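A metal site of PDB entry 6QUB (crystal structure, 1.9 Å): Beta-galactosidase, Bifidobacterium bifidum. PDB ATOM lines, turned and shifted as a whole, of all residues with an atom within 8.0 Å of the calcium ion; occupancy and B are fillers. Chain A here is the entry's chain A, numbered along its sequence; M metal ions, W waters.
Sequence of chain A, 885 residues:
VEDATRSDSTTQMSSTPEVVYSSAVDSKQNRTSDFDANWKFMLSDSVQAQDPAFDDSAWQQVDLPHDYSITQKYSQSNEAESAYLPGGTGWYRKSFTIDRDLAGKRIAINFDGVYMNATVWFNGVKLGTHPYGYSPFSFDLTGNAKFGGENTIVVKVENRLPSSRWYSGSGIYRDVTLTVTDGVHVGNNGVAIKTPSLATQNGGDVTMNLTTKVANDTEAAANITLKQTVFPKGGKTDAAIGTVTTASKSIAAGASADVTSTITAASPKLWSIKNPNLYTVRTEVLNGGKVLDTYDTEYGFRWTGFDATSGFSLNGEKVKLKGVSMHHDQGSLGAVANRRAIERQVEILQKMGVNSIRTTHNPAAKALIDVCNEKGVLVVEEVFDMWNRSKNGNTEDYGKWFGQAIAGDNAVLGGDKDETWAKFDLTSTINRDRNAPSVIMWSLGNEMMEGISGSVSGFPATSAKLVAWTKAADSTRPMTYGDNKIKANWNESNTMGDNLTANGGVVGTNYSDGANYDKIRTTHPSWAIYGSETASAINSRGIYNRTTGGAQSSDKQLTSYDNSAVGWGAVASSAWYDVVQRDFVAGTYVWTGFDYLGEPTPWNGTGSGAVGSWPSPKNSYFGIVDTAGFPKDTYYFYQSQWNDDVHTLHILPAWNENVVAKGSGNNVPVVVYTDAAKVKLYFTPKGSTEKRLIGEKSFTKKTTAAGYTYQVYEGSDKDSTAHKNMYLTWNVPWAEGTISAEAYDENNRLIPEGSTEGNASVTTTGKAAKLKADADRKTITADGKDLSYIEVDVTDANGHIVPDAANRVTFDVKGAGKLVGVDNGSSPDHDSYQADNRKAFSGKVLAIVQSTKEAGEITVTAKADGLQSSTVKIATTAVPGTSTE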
ATOM      1  N   GLU A  79       6.761 -33.088  -9.475  1.00  0.00           N
ATOM      2  CA  GLU A  79       6.841 -32.221 -10.646  1.00  0.00           C
ATOM      3  C   GLU A  79       8.021 -31.258 -10.540  1.00  0.00           C
ATOM      4  O   GLU A  79       8.264 -30.674  -9.477  1.00  0.00           O
ATOM      5  CB  GLU A  79       5.530 -31.446 -10.842  1.00  0.00           C
ATOM      6  CG  GLU A  79       4.335 -32.385 -11.021  1.00  0.00           C
ATOM      7  CD  GLU A  79       3.061 -31.680 -11.450  1.00  0.00           C
ATOM      8  OE1 GLU A  79       3.035 -30.431 -11.473  1.00  0.00           O
ATOM      9  OE2 GLU A  79       2.071 -32.372 -11.764  1.00  0.00           O
ATOM     10  N   ALA A  80       8.752 -31.117 -11.640  1.00  0.00           N
ATOM     11  CA  ALA A  80       9.934 -30.255 -11.653  1.00  0.00           C
ATOM     12  C   ALA A  80       9.567 -28.812 -11.322  1.00  0.00           C
ATOM     13  O   ALA A  80      10.316 -28.129 -10.612  1.00  0.00           O
ATOM     14  CB  ALA A  80      10.627 -30.321 -13.017  1.00  0.00           C
ATOM     15  N   GLU A  81       8.439 -28.330 -11.832  1.00  0.00           N
ATOM     16  CA  GLU A  81       8.098 -26.925 -11.649  1.00  0.00           C
ATOM     17  C   GLU A  81       7.958 -26.568 -10.172  1.00  0.00           C
ATOM     18  O   GLU A  81       8.155 -25.416  -9.797  1.00  0.00           O
ATOM     19  CB  GLU A  81       6.811 -26.587 -12.414  1.00  0.00           C
ATOM     20  CG  GLU A  81       5.572 -27.282 -11.893  1.00  0.00           C
ATOM     21  CD  GLU A  81       4.303 -26.789 -12.570  1.00  0.00           C
ATOM     22  OE1 GLU A  81       4.380 -25.944 -13.487  1.00  0.00           O
ATOM     23  OE2 GLU A  81       3.220 -27.253 -12.155  1.00  0.00           O
ATOM     24  N   SER A  82       7.610 -27.541  -9.322  1.00  0.00           N
ATOM     25  CA  SER A  82       7.528 -27.309  -7.888  1.00  0.00           C
ATOM     26  C   SER A  82       8.655 -28.022  -7.134  1.00  0.00           C
ATOM     27  O   SER A  82       8.487 -28.399  -5.973  1.00  0.00           O
ATOM     28  CB  SER A  82       6.157 -27.715  -7.357  1.00  0.00           C
ATOM     29  OG  SER A  82       5.758 -28.973  -7.852  1.00  0.00           O
ATOM     30  N   LEU A 161      -1.075 -31.274  -4.331  1.00  0.00           N
ATOM     31  CA  LEU A 161      -0.425 -30.948  -5.590  1.00  0.00           C
ATOM     32  C   LEU A 161      -1.266 -31.488  -6.751  1.00  0.00           C
ATOM     33  O   LEU A 161      -1.987 -32.462  -6.578  1.00  0.00           O
ATOM     34  CB  LEU A 161       0.986 -31.525  -5.628  1.00  0.00           C
ATOM     35  CG  LEU A 161       1.920 -31.034  -4.521  1.00  0.00           C
ATOM     36  CD1 LEU A 161       3.368 -31.255  -4.926  1.00  0.00           C
ATOM     37  CD2 LEU A 161       1.673 -29.567  -4.175  1.00  0.00           C
ATOM     38  N   PRO A 162      -1.174 -30.857  -7.933  1.00  0.00           N
ATOM     39  CA  PRO A 162      -0.348 -29.691  -8.276  1.00  0.00           C
ATOM     40  C   PRO A 162      -1.074 -28.362  -8.072  1.00  0.00           C
ATOM     41  O   PRO A 162      -2.220 -28.215  -8.493  1.00  0.00           O
ATOM     42  CB  PRO A 162      -0.027 -29.927  -9.745  1.00  0.00           C
ATOM     43  CG  PRO A 162      -1.264 -30.591 -10.261  1.00  0.00           C
ATOM     44  CD  PRO A 162      -1.868 -31.378  -9.119  1.00  0.00           C
ATOM     45  N   SER A 163      -0.399 -27.397  -7.457  1.00  0.00           N
ATOM     46  CA  SER A 163      -1.049 -26.137  -7.133  1.00  0.00           C
ATOM     47  C   SER A 163      -0.214 -24.909  -7.466  1.00  0.00           C
ATOM     48  O   SER A 163      -0.615 -23.794  -7.095  1.00  0.00           O
ATOM     49  CB  SER A 163      -1.419 -26.098  -5.650  1.00  0.00           C
ATOM     50  OG  SER A 163      -0.258 -26.028  -4.848  1.00  0.00           O
ATOM     51  N   SER A 164       0.931 -25.058  -8.128  1.00  0.00           N
ATOM     52  CA  SER A 164       1.813 -23.911  -8.275  1.00  0.00           C
ATOM     53  C   SER A 164       2.746 -24.124  -9.465  1.00  0.00           C
ATOM     54  O   SER A 164       3.178 -25.245  -9.731  1.00  0.00           O
ATOM     55  CB  SER A 164       2.633 -23.700  -6.993  1.00  0.00           C
ATOM     56  OG  SER A 164       3.367 -22.495  -7.041  1.00  0.00           O
ATOM     57  N   ARG A 165       3.044 -23.030 -10.171  1.00  0.00           N
ATOM     58  CA  ARG A 165       4.066 -23.037 -11.206  1.00  0.00           C
ATOM     59  C   ARG A 165       5.483 -22.912 -10.639  1.00  0.00           C
ATOM     60  O   ARG A 165       6.444 -22.981 -11.419  1.00  0.00           O
ATOM     61  CB  ARG A 165       3.811 -21.911 -12.218  1.00  0.00           C
ATOM     62  CG  ARG A 165       2.522 -22.052 -13.012  1.00  0.00           C
ATOM     63  CD  ARG A 165       2.407 -20.999 -14.128  1.00  0.00           C
ATOM     64  NE  ARG A 165       2.455 -19.627 -13.613  1.00  0.00           N
ATOM     65  CZ  ARG A 165       3.496 -18.810 -13.749  1.00  0.00           C
ATOM     66  NH1 ARG A 165       4.588 -19.214 -14.390  1.00  0.00           N
ATOM     67  NH2 ARG A 165       3.447 -17.578 -13.256  1.00  0.00           N
ATOM     68  N   LYS A 391      -3.492 -22.814 -14.356  1.00  0.00           N
ATOM     69  CA  LYS A 391      -2.364 -22.813 -15.275  1.00  0.00           C
ATOM     70  C   LYS A 391      -1.605 -24.133 -15.243  1.00  0.00           C
ATOM     71  O   LYS A 391      -1.532 -24.798 -14.201  1.00  0.00           O
ATOM     72  CB  LYS A 391      -1.382 -21.682 -14.935  1.00  0.00           C
ATOM     73  CG  LYS A 391      -1.926 -20.287 -15.184  1.00  0.00           C
ATOM     74  CD  LYS A 391      -0.866 -19.266 -14.803  1.00  0.00           C
ATOM     75  CE  LYS A 391      -1.230 -17.889 -15.292  1.00  0.00           C
ATOM     76  NZ  LYS A 391      -0.089 -16.945 -15.113  1.00  0.00           N
ATOM     77  N   ASN A 392      -1.039 -24.495 -16.391  1.00  0.00           N
ATOM     78  CA  ASN A 392      -0.030 -25.554 -16.466  1.00  0.00           C
ATOM     79  C   ASN A 392      -0.529 -26.881 -15.888  1.00  0.00           C
ATOM     80  O   ASN A 392       0.254 -27.635 -15.307  1.00  0.00           O
ATOM     81  CB  ASN A 392       1.263 -25.129 -15.753  1.00  0.00           C
ATOM     82  CG  ASN A 392       1.970 -23.956 -16.451  1.00  0.00           C
ATOM     83  OD1 ASN A 392       1.424 -23.306 -17.333  1.00  0.00           O
ATOM     84  ND2 ASN A 392       3.205 -23.699 -16.032  1.00  0.00           N
ATOM     85  N   GLY A 393      -1.833 -27.161 -16.002  1.00  0.00           N
ATOM     86  CA  GLY A 393      -2.361 -28.387 -15.443  1.00  0.00           C
ATOM     87  C   GLY A 393      -2.380 -28.450 -13.932  1.00  0.00           C
ATOM     88  O   GLY A 393      -2.534 -29.544 -13.361  1.00  0.00           O
ATOM     89  N   ASN A 394      -2.226 -27.310 -13.260  1.00  0.00           N
ATOM     90  CA  ASN A 394      -2.218 -27.262 -11.793  1.00  0.00           C
ATOM     91  C   ASN A 394      -3.661 -27.118 -11.316  1.00  0.00           C
ATOM     92  O   ASN A 394      -4.132 -26.025 -10.987  1.00  0.00           O
ATOM     93  CB  ASN A 394      -1.341 -26.108 -11.309  1.00  0.00           C
ATOM     94  CG  ASN A 394       0.115 -26.323 -11.661  1.00  0.00           C
ATOM     95  OD1 ASN A 394       0.566 -27.456 -11.769  1.00  0.00           O
ATOM     96  ND2 ASN A 394       0.862 -25.222 -11.844  1.00  0.00           N
ATOM     97  N   THR A 395      -4.362 -28.251 -11.303  1.00  0.00           N
ATOM     98  CA  THR A 395      -5.800 -28.232 -11.047  1.00  0.00           C
ATOM     99  C   THR A 395      -6.136 -27.803  -9.624  1.00  0.00           C
ATOM    100  O   THR A 395      -7.287 -27.444  -9.352  1.00  0.00           O
ATOM    101  CB  THR A 395      -6.402 -29.623 -11.299  1.00  0.00           C
ATOM    102  OG1 THR A 395      -5.773 -30.590 -10.445  1.00  0.00           O
ATOM    103  CG2 THR A 395      -6.213 -30.024 -12.749  1.00  0.00           C
ATOM    104  N   ASP A 397      -4.446 -25.266  -8.098  1.00  0.00           N
ATOM    105  CA  ASP A 397      -3.984 -23.914  -7.850  1.00  0.00           C
ATOM    106  C   ASP A 397      -5.184 -23.004  -7.545  1.00  0.00           C
ATOM    107  O   ASP A 397      -6.336 -23.459  -7.453  1.00  0.00           O
ATOM    108  CB  ASP A 397      -3.122 -23.403  -9.004  1.00  0.00           C
ATOM    109  CG  ASP A 397      -3.897 -23.105 -10.283  1.00  0.00           C
ATOM    110  OD1 ASP A 397      -5.142 -22.960 -10.264  1.00  0.00           O
ATOM    111  OD2 ASP A 397      -3.230 -22.986 -11.338  1.00  0.00           O
ATOM    112  N   GLY A 605       9.397 -28.870 -16.056  1.00  0.00           N
ATOM    113  CA  GLY A 605       8.439 -29.901 -16.333  1.00  0.00           C
ATOM    114  C   GLY A 605       7.145 -29.594 -15.608  1.00  0.00           C
ATOM    115  O   GLY A 605       7.121 -29.518 -14.383  1.00  0.00           O
ATOM    116  N   THR A 606       6.073 -29.350 -16.365  1.00  0.00           N
ATOM    117  CA  THR A 606       4.786 -29.058 -15.743  1.00  0.00           C
ATOM    118  C   THR A 606       4.005 -30.312 -15.371  1.00  0.00           C
ATOM    119  O   THR A 606       2.959 -30.201 -14.725  1.00  0.00           O
ATOM    120  CB  THR A 606       3.936 -28.166 -16.661  1.00  0.00           C
ATOM    121  OG1 THR A 606       3.772 -28.813 -17.929  1.00  0.00           O
ATOM    122  CG2 THR A 606       4.621 -26.820 -16.854  1.00  0.00           C
ATOM    123  N   GLY A 607       4.476 -31.507 -15.759  1.00  0.00           N
ATOM    124  CA  GLY A 607       3.934 -32.750 -15.292  1.00  0.00           C
ATOM    125  C   GLY A 607       4.901 -33.502 -14.398  1.00  0.00           C
ATOM    126  O   GLY A 607       5.867 -32.940 -13.868  1.00  0.00           O
ATOM    127  N   SER A 608       4.645 -34.795 -14.230  1.00  0.00           N
ATOM    128  CA  SER A 608       5.492 -35.622 -13.382  1.00  0.00           C
ATOM    129  C   SER A 608       6.687 -36.148 -14.181  1.00  0.00           C
ATOM    130  O   SER A 608       6.732 -36.060 -15.413  1.00  0.00           O
ATOM    131  CB  SER A 608       4.704 -36.774 -12.787  1.00  0.00           C
ATOM    132  OG  SER A 608       4.454 -37.767 -13.769  1.00  0.00           O
HETATM  133 CA    CA M   1       1.810 -28.806 -13.231  1.00  0.00          CA
HETATM  134  O   HOH W   1       0.371 -30.572 -13.121  1.00  0.00           O
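The calcium ion is bound by water W1. O of Thr 606 is bound to the calcium ion (2.3 Å). The calcium ion is bound by the side-chain amide oxygen (OD1) of Asn 394, 2.3 Å away. OE2 of Glu 81 is bound to the calcium ion, at 2.4 Å. The calcium ion is bound by OE1 of Glu 79 (2.7 Å). The calcium ion is bound by the backbone carbonyl oxygen (O) of Asn 392, 2.8 Å away.
O of Lys 391 lies close to ND2 of Asn 394, at 3.4 Å. O of Gly 605 sits at hydrogen-bond distance from N of Glu 81 (3.1 Å). The side-chain hydroxyl (OG) of Ser 82 lies within hydrogen-bond range of the backbone carbonyl oxygen (O) of Glu 79 (3.4 Å). The side-chain amide nitrogen of Asn 394 sits at hydrogen-bond distance from the backbone carbonyl oxygen of Ser 164 (3.1 Å).
Water W1 bridges OE2 of Glu 79 (2.8 Å) and O of Gly 393 (3.1 Å).
Of the 19 residues printed, 5 come within 4 Å of the calcium ion. The nearest printed residue that does not touch the calcium ion is Pro 162 (4.1 Å).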
